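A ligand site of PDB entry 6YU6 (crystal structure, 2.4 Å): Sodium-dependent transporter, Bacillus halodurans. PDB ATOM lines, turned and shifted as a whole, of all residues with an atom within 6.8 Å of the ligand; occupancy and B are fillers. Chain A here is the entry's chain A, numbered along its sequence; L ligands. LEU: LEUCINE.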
ATOM      1  N   GLY A  26     -37.176 -12.180  26.643  1.00  0.00           N
ATOM      2  CA  GLY A  26     -36.529 -13.388  27.133  1.00  0.00           C
ATOM      3  C   GLY A  26     -35.620 -14.018  26.103  1.00  0.00           C
ATOM      4  O   GLY A  26     -34.659 -14.698  26.445  1.00  0.00           O
ATOM      5  N   SER A  27     -35.912 -13.811  24.816  1.00  0.00           N
ATOM      6  CA  SER A  27     -35.025 -14.281  23.761  1.00  0.00           C
ATOM      7  C   SER A  27     -33.785 -13.411  23.644  1.00  0.00           C
ATOM      8  O   SER A  27     -32.681 -13.919  23.448  1.00  0.00           O
ATOM      9  CB  SER A  27     -35.773 -14.319  22.427  1.00  0.00           C
ATOM     10  OG  SER A  27     -34.884 -14.586  21.361  1.00  0.00           O
ATOM     11  N   ALA A  28     -33.955 -12.089  23.774  1.00  0.00           N
ATOM     12  CA  ALA A  28     -32.848 -11.169  23.549  1.00  0.00           C
ATOM     13  C   ALA A  28     -31.889 -11.125  24.728  1.00  0.00           C
ATOM     14  O   ALA A  28     -30.675 -11.060  24.532  1.00  0.00           O
ATOM     15  CB  ALA A  28     -33.395  -9.770  23.244  1.00  0.00           C
ATOM     16  N   VAL A  29     -32.406 -11.153  25.954  1.00  0.00           N
ATOM     17  CA  VAL A  29     -31.591 -10.989  27.146  1.00  0.00           C
ATOM     18  C   VAL A  29     -31.052 -12.349  27.565  1.00  0.00           C
ATOM     19  O   VAL A  29     -31.783 -13.178  28.111  1.00  0.00           O
ATOM     20  CB  VAL A  29     -32.394 -10.336  28.289  1.00  0.00           C
ATOM     21  CG1 VAL A  29     -31.514 -10.158  29.516  1.00  0.00           C
ATOM     22  CG2 VAL A  29     -32.956  -9.004  27.829  1.00  0.00           C
ATOM     23  N   GLY A  30     -29.772 -12.585  27.306  1.00  0.00           N
ATOM     24  CA  GLY A  30     -29.139 -13.841  27.629  1.00  0.00           C
ATOM     25  C   GLY A  30     -27.643 -13.741  27.808  1.00  0.00           C
ATOM     26  O   GLY A  30     -27.149 -12.787  28.399  1.00  0.00           O
ATOM     27  N   LEU A  31     -26.907 -14.725  27.279  1.00  0.00           N
ATOM     28  CA  LEU A  31     -25.461 -14.762  27.480  1.00  0.00           C
ATOM     29  C   LEU A  31     -24.726 -13.752  26.611  1.00  0.00           C
ATOM     30  O   LEU A  31     -23.583 -13.406  26.927  1.00  0.00           O
ATOM     31  CB  LEU A  31     -24.922 -16.168  27.216  1.00  0.00           C
ATOM     32  CG  LEU A  31     -25.146 -17.057  28.434  1.00  0.00           C
ATOM     33  CD1 LEU A  31     -24.537 -18.434  28.157  1.00  0.00           C
ATOM     34  CD2 LEU A  31     -24.467 -16.431  29.648  1.00  0.00           C
ATOM     35  N   GLY A  32     -25.341 -13.285  25.528  1.00  0.00           N
ATOM     36  CA  GLY A  32     -24.692 -12.324  24.659  1.00  0.00           C
ATOM     37  C   GLY A  32     -24.515 -10.957  25.289  1.00  0.00           C
ATOM     38  O   GLY A  32     -23.687 -10.176  24.815  1.00  0.00           O
ATOM     39  N   ASN A  33     -25.255 -10.654  26.352  1.00  0.00           N
ATOM     40  CA  ASN A  33     -25.182  -9.347  26.975  1.00  0.00           C
ATOM     41  C   ASN A  33     -24.022  -9.230  27.957  1.00  0.00           C
ATOM     42  O   ASN A  33     -23.441  -8.157  28.092  1.00  0.00           O
ATOM     43  CB  ASN A  33     -26.498  -9.045  27.707  1.00  0.00           C
ATOM     44  CG  ASN A  33     -27.695  -9.078  26.792  1.00  0.00           C
ATOM     45  OD1 ASN A  33     -28.235 -10.158  26.495  1.00  0.00           O
ATOM     46  ND2 ASN A  33     -28.128  -7.918  26.325  1.00  0.00           N
ATOM     47  N   ILE A  34     -23.674 -10.318  28.643  1.00  0.00           N
ATOM     48  CA  ILE A  34     -22.654 -10.303  29.685  1.00  0.00           C
ATOM     49  C   ILE A  34     -21.405 -11.047  29.249  1.00  0.00           C
ATOM     50  O   ILE A  34     -20.305 -10.494  29.265  1.00  0.00           O
ATOM     51  CB  ILE A  34     -23.207 -10.861  31.021  1.00  0.00           C
ATOM     52  CG1 ILE A  34     -24.382 -10.014  31.520  1.00  0.00           C
ATOM     53  CG2 ILE A  34     -22.107 -10.937  32.062  1.00  0.00           C
ATOM     54  CD1 ILE A  34     -25.739 -10.549  31.127  1.00  0.00           C
ATOM     55  N   ILE A 106     -25.427 -21.620  16.303  1.00  0.00           N
ATOM     56  CA  ILE A 106     -25.270 -20.820  17.508  1.00  0.00           C
ATOM     57  C   ILE A 106     -25.698 -21.599  18.739  1.00  0.00           C
ATOM     58  O   ILE A 106     -25.014 -21.559  19.781  1.00  0.00           O
ATOM     59  CB  ILE A 106     -26.063 -19.507  17.367  1.00  0.00           C
ATOM     60  CG1 ILE A 106     -25.324 -18.547  16.423  1.00  0.00           C
ATOM     61  CG2 ILE A 106     -26.276 -18.867  18.730  1.00  0.00           C
ATOM     62  CD1 ILE A 106     -26.140 -17.354  15.992  1.00  0.00           C
ATOM     63  N   LEU A 107     -26.802 -22.343  18.649  1.00  0.00           N
ATOM     64  CA  LEU A 107     -27.261 -23.117  19.800  1.00  0.00           C
ATOM     65  C   LEU A 107     -26.233 -24.172  20.210  1.00  0.00           C
ATOM     66  O   LEU A 107     -26.147 -24.529  21.396  1.00  0.00           O
ATOM     67  CB  LEU A 107     -28.607 -23.776  19.487  1.00  0.00           C
ATOM     68  CG  LEU A 107     -29.183 -24.484  20.713  1.00  0.00           C
ATOM     69  CD1 LEU A 107     -29.527 -23.449  21.785  1.00  0.00           C
ATOM     70  CD2 LEU A 107     -30.450 -25.240  20.328  1.00  0.00           C
ATOM     71  N   TYR A 110     -23.769 -22.294  22.234  1.00  0.00           N
ATOM     72  CA  TYR A 110     -24.456 -21.552  23.274  1.00  0.00           C
ATOM     73  C   TYR A 110     -24.684 -22.415  24.507  1.00  0.00           C
ATOM     74  O   TYR A 110     -24.495 -21.973  25.638  1.00  0.00           O
ATOM     75  CB  TYR A 110     -25.786 -21.012  22.745  1.00  0.00           C
ATOM     76  CG  TYR A 110     -26.356 -19.842  23.508  1.00  0.00           C
ATOM     77  CD1 TYR A 110     -26.020 -18.535  23.170  1.00  0.00           C
ATOM     78  CD2 TYR A 110     -27.241 -20.029  24.558  1.00  0.00           C
ATOM     79  CE1 TYR A 110     -26.551 -17.465  23.855  1.00  0.00           C
ATOM     80  CE2 TYR A 110     -27.773 -18.964  25.252  1.00  0.00           C
ATOM     81  CZ  TYR A 110     -27.423 -17.682  24.900  1.00  0.00           C
ATOM     82  OH  TYR A 110     -27.943 -16.612  25.587  1.00  0.00           O
ATOM     83  N   GLN A 229     -21.860  -8.532  17.192  1.00  0.00           N
ATOM     84  CA  GLN A 229     -22.425  -8.426  18.536  1.00  0.00           C
ATOM     85  C   GLN A 229     -23.789  -7.749  18.498  1.00  0.00           C
ATOM     86  O   GLN A 229     -24.670  -8.086  19.301  1.00  0.00           O
ATOM     87  CB  GLN A 229     -21.477  -7.665  19.443  1.00  0.00           C
ATOM     88  CG  GLN A 229     -21.977  -7.502  20.871  1.00  0.00           C
ATOM     89  CD  GLN A 229     -22.156  -8.828  21.579  1.00  0.00           C
ATOM     90  OE1 GLN A 229     -21.472  -9.800  21.284  1.00  0.00           O
ATOM     91  NE2 GLN A 229     -23.100  -8.876  22.508  1.00  0.00           N
ATOM     92  N   PHE A 231     -26.158  -7.960  16.104  1.00  0.00           N
ATOM     93  CA  PHE A 231     -27.181  -8.915  15.692  1.00  0.00           C
ATOM     94  C   PHE A 231     -27.296 -10.084  16.655  1.00  0.00           C
ATOM     95  O   PHE A 231     -28.382 -10.631  16.840  1.00  0.00           O
ATOM     96  CB  PHE A 231     -26.893  -9.433  14.277  1.00  0.00           C
ATOM     97  CG  PHE A 231     -27.169  -8.436  13.175  1.00  0.00           C
ATOM     98  CD1 PHE A 231     -27.041  -7.070  13.397  1.00  0.00           C
ATOM     99  CD2 PHE A 231     -27.548  -8.865  11.923  1.00  0.00           C
ATOM    100  CE1 PHE A 231     -27.291  -6.170  12.392  1.00  0.00           C
ATOM    101  CE2 PHE A 231     -27.795  -7.968  10.905  1.00  0.00           C
ATOM    102  CZ  PHE A 231     -27.667  -6.621  11.139  1.00  0.00           C
ATOM    103  N   PHE A 232     -26.186 -10.474  17.288  1.00  0.00           N
ATOM    104  CA  PHE A 232     -26.213 -11.584  18.234  1.00  0.00           C
ATOM    105  C   PHE A 232     -27.039 -11.238  19.465  1.00  0.00           C
ATOM    106  O   PHE A 232     -27.890 -12.014  19.883  1.00  0.00           O
ATOM    107  CB  PHE A 232     -24.780 -11.964  18.631  1.00  0.00           C
ATOM    108  CG  PHE A 232     -24.703 -13.203  19.488  1.00  0.00           C
ATOM    109  CD1 PHE A 232     -24.785 -13.118  20.868  1.00  0.00           C
ATOM    110  CD2 PHE A 232     -24.523 -14.447  18.908  1.00  0.00           C
ATOM    111  CE1 PHE A 232     -24.708 -14.251  21.658  1.00  0.00           C
ATOM    112  CE2 PHE A 232     -24.446 -15.589  19.694  1.00  0.00           C
ATOM    113  CZ  PHE A 232     -24.538 -15.486  21.060  1.00  0.00           C
ATOM    114  N   THR A 233     -26.787 -10.064  20.048  1.00  0.00           N
ATOM    115  CA  THR A 233     -27.502  -9.688  21.259  1.00  0.00           C
ATOM    116  C   THR A 233     -28.984  -9.423  21.012  1.00  0.00           C
ATOM    117  O   THR A 233     -29.783  -9.506  21.943  1.00  0.00           O
ATOM    118  CB  THR A 233     -26.848  -8.454  21.894  1.00  0.00           C
ATOM    119  OG1 THR A 233     -27.317  -8.284  23.236  1.00  0.00           O
ATOM    120  CG2 THR A 233     -27.157  -7.190  21.092  1.00  0.00           C
ATOM    121  N   LEU A 234     -29.369  -9.128  19.768  1.00  0.00           N
ATOM    122  CA  LEU A 234     -30.749  -8.830  19.408  1.00  0.00           C
ATOM    123  C   LEU A 234     -31.513 -10.053  18.909  1.00  0.00           C
ATOM    124  O   LEU A 234     -32.698  -9.932  18.591  1.00  0.00           O
ATOM    125  CB  LEU A 234     -30.795  -7.745  18.339  1.00  0.00           C
ATOM    126  CG  LEU A 234     -30.535  -6.360  18.940  1.00  0.00           C
ATOM    127  CD1 LEU A 234     -30.855  -5.298  17.895  1.00  0.00           C
ATOM    128  CD2 LEU A 234     -31.419  -6.150  20.170  1.00  0.00           C
ATOM    129  N   SER A 235     -30.857 -11.218  18.825  1.00  0.00           N
ATOM    130  CA  SER A 235     -31.466 -12.433  18.296  1.00  0.00           C
ATOM    131  C   SER A 235     -31.917 -12.258  16.852  1.00  0.00           C
ATOM    132  O   SER A 235     -32.921 -12.842  16.422  1.00  0.00           O
ATOM    133  CB  SER A 235     -32.635 -12.910  19.160  1.00  0.00           C
ATOM    134  OG  SER A 235     -32.214 -13.169  20.497  1.00  0.00           O
ATOM    135  N   LEU A 236     -31.174 -11.463  16.080  1.00  0.00           N
ATOM    136  CA  LEU A 236     -31.477 -11.198  14.686  1.00  0.00           C
ATOM    137  C   LEU A 236     -30.706 -12.149  13.775  1.00  0.00           C
ATOM    138  O   LEU A 236     -29.623 -12.633  14.133  1.00  0.00           O
ATOM    139  CB  LEU A 236     -31.150  -9.747  14.314  1.00  0.00           C
ATOM    140  CG  LEU A 236     -32.126  -8.798  15.001  1.00  0.00           C
ATOM    141  CD1 LEU A 236     -31.713  -7.362  14.684  1.00  0.00           C
ATOM    142  CD2 LEU A 236     -33.535  -9.035  14.474  1.00  0.00           C
ATOM    143  N   MET A 238     -31.307 -15.142  12.972  1.00  0.00           N
ATOM    144  CA  MET A 238     -31.377 -16.546  13.355  1.00  0.00           C
ATOM    145  C   MET A 238     -32.808 -17.066  13.368  1.00  0.00           C
ATOM    146  O   MET A 238     -33.078 -18.121  13.958  1.00  0.00           O
ATOM    147  CB  MET A 238     -30.710 -16.755  14.715  1.00  0.00           C
ATOM    148  CG  MET A 238     -31.208 -15.803  15.785  1.00  0.00           C
ATOM    149  SD  MET A 238     -30.053 -15.627  17.159  1.00  0.00           S
ATOM    150  CE  MET A 238     -28.696 -14.766  16.366  1.00  0.00           C
ATOM    151  N   ALA A 240     -35.337 -16.135  14.980  1.00  0.00           N
ATOM    152  CA  ALA A 240     -35.997 -16.149  16.284  1.00  0.00           C
ATOM    153  C   ALA A 240     -37.176 -15.187  16.329  1.00  0.00           C
ATOM    154  O   ALA A 240     -38.290 -15.579  16.704  1.00  0.00           O
ATOM    155  CB  ALA A 240     -34.984 -15.808  17.383  1.00  0.00           C
ATOM    156  N   ASP A 265     -32.569  -4.367  26.242  1.00  0.00           N
ATOM    157  CA  ASP A 265     -31.372  -5.184  26.027  1.00  0.00           C
ATOM    158  C   ASP A 265     -30.116  -4.336  26.119  1.00  0.00           C
ATOM    159  O   ASP A 265     -29.144  -4.714  26.794  1.00  0.00           O
ATOM    160  CB  ASP A 265     -31.459  -5.895  24.682  1.00  0.00           C
ATOM    161  CG  ASP A 265     -30.250  -6.758  24.407  1.00  0.00           C
ATOM    162  OD1 ASP A 265     -30.127  -7.834  25.026  1.00  0.00           O
ATOM    163  OD2 ASP A 265     -29.421  -6.361  23.565  1.00  0.00           O
ATOM    164  N   ALA A 322     -31.963 -16.612  32.208  1.00  0.00           N
ATOM    165  CA  ALA A 322     -31.979 -15.783  31.006  1.00  0.00           C
ATOM    166  C   ALA A 322     -31.272 -16.468  29.850  1.00  0.00           C
ATOM    167  O   ALA A 322     -31.675 -16.314  28.686  1.00  0.00           O
ATOM    168  CB  ALA A 322     -31.341 -14.423  31.286  1.00  0.00           C
ATOM    169  N   ALA A 323     -30.215 -17.231  30.139  1.00  0.00           N
ATOM    170  CA  ALA A 323     -29.602 -18.057  29.104  1.00  0.00           C
ATOM    171  C   ALA A 323     -30.507 -19.208  28.704  1.00  0.00           C
ATOM    172  O   ALA A 323     -30.470 -19.672  27.555  1.00  0.00           O
ATOM    173  CB  ALA A 323     -28.246 -18.582  29.574  1.00  0.00           C
ATOM    174  N   SER A 325     -33.849 -18.992  28.557  1.00  0.00           N
ATOM    175  CA  SER A 325     -34.883 -18.444  27.685  1.00  0.00           C
ATOM    176  C   SER A 325     -34.335 -18.092  26.301  1.00  0.00           C
ATOM    177  O   SER A 325     -35.077 -18.132  25.324  1.00  0.00           O
ATOM    178  CB  SER A 325     -35.514 -17.217  28.326  1.00  0.00           C
ATOM    179  OG  SER A 325     -34.519 -16.291  28.742  1.00  0.00           O
ATOM    180  N   SER A 326     -33.049 -17.750  26.210  1.00  0.00           N
ATOM    181  CA  SER A 326     -32.470 -17.416  24.909  1.00  0.00           C
ATOM    182  C   SER A 326     -32.237 -18.675  24.083  1.00  0.00           C
ATOM    183  O   SER A 326     -32.427 -18.677  22.869  1.00  0.00           O
ATOM    184  CB  SER A 326     -31.169 -16.634  25.093  1.00  0.00           C
ATOM    185  OG  SER A 326     -31.410 -15.374  25.666  1.00  0.00           O
ATOM    186  N   ALA A 327     -31.814 -19.768  24.737  1.00  0.00           N
ATOM    187  CA  ALA A 327     -31.617 -21.018  24.029  1.00  0.00           C
ATOM    188  C   ALA A 327     -32.945 -21.649  23.629  1.00  0.00           C
ATOM    189  O   ALA A 327     -33.024 -22.323  22.594  1.00  0.00           O
ATOM    190  CB  ALA A 327     -30.816 -21.988  24.885  1.00  0.00           C
ATOM    191  N   SER A 329     -35.506 -19.960  22.625  1.00  0.00           N
ATOM    192  CA  SER A 329     -35.828 -19.263  21.384  1.00  0.00           C
ATOM    193  C   SER A 329     -34.942 -19.715  20.235  1.00  0.00           C
ATOM    194  O   SER A 329     -35.344 -19.574  19.075  1.00  0.00           O
ATOM    195  CB  SER A 329     -35.709 -17.753  21.572  1.00  0.00           C
ATOM    196  OG  SER A 329     -34.379 -17.384  21.904  1.00  0.00           O
ATOM    197  N   LEU A 330     -33.755 -20.249  20.526  1.00  0.00           N
ATOM    198  CA  LEU A 330     -32.920 -20.823  19.477  1.00  0.00           C
ATOM    199  C   LEU A 330     -33.474 -22.166  19.006  1.00  0.00           C
ATOM    200  O   LEU A 330     -33.593 -22.410  17.809  1.00  0.00           O
ATOM    201  CB  LEU A 330     -31.488 -21.005  19.975  1.00  0.00           C
ATOM    202  CG  LEU A 330     -30.748 -19.670  20.018  1.00  0.00           C
ATOM    203  CD1 LEU A 330     -29.614 -19.769  21.048  1.00  0.00           C
ATOM    204  CD2 LEU A 330     -30.146 -19.376  18.650  1.00  0.00           C
HETATM  205  N   LEU L   1     -29.856 -12.851  21.948  1.00  0.00           N
HETATM  206  CA  LEU L   1     -29.243 -13.819  22.849  1.00  0.00           C
HETATM  207  C   LEU L   1     -28.310 -13.118  23.836  1.00  0.00           C
HETATM  208  O   LEU L   1     -27.735 -13.779  24.736  1.00  0.00           O
HETATM  209  CB  LEU L   1     -28.468 -14.874  22.063  1.00  0.00           C
HETATM  210  CG  LEU L   1     -29.325 -15.440  20.940  1.00  0.00           C
HETATM  211  CD1 LEU L   1     -28.466 -16.428  20.164  1.00  0.00           C
HETATM  212  CD2 LEU L   1     -30.536 -16.174  21.527  1.00  0.00           C
HETATM  213  OXT LEU L   1     -28.098 -11.878  23.727  1.00  0.00           O
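CG2 of Ile 106 touches CD1 of the ligand (3.6 Å). Met 238 touches the ligand. Ser 326 touches the ligand (O to CD2, 3.4 Å). CD1 of Leu 330 touches CD1 of the ligand, at 3.6 Å.
An oxygen (O) of the ligand is in hydrogen-bond range of the backbone NH (N) of Gly 32 (2.6 Å). A nitrogen (N) of the ligand lies within hydrogen-bond range of the side-chain hydroxyl (OG) of Ser 235 (2.8 Å). The backbone carbonyl oxygen (O) of Ala 28 sits close to a nitrogen (N) of the ligand (3.2 Å). An oxygen (O) of the ligand lies within hydrogen-bond range of the backbone NH (N) of Leu 31 (2.8 Å). OH of Tyr 110 sits at hydrogen-bond distance from O of the ligand (3.0 Å). The backbone carbonyl oxygen (O) of Phe 232 lies within hydrogen-bond range of a nitrogen (N) of the ligand (3.0 Å). The backbone NH of Gly 30 sits close to an oxygen (O) of the ligand. The side-chain amide oxygen of Asn 33 lies close to an oxygen (OXT) of the ligand, 3.3 Å away. O of Thr 233 lies within hydrogen-bond range of N of the ligand (3.3 Å). O of Ser 27 sits at hydrogen-bond distance from N of the ligand (3.4 Å).
The side-chain hydroxyl of Ser 235 sits at hydrogen-bond distance from the backbone carbonyl oxygen of Ser 27 (3.1 Å). The backbone NH (N) of Leu 31 lies within hydrogen-bond range of the side-chain hydroxyl (OH) of Tyr 110, 2.7 Å away. ND2 of Asn 33 is in hydrogen-bond range of OG1 of Thr 233. OD1 of Asn 33 lies close to OD1 of Asp 265 (3.3 Å). The side-chain hydroxyl (OG) of Ser 326 is in hydrogen-bond range of the backbone carbonyl oxygen (O) of Ser 27, 2.9 Å away. The backbone carbonyl oxygen (O) of Ser 326 is in hydrogen-bond range of the side-chain hydroxyl (OG) of Ser 329, 2.5 Å away. The side-chain hydroxyl (OG) of Ser 326 lies within hydrogen-bond range of the backbone carbonyl oxygen (O) of Ala 322, at 3.2 Å. OG of Ser 326 lies within hydrogen-bond range of O of Gly 26 (3.4 Å).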
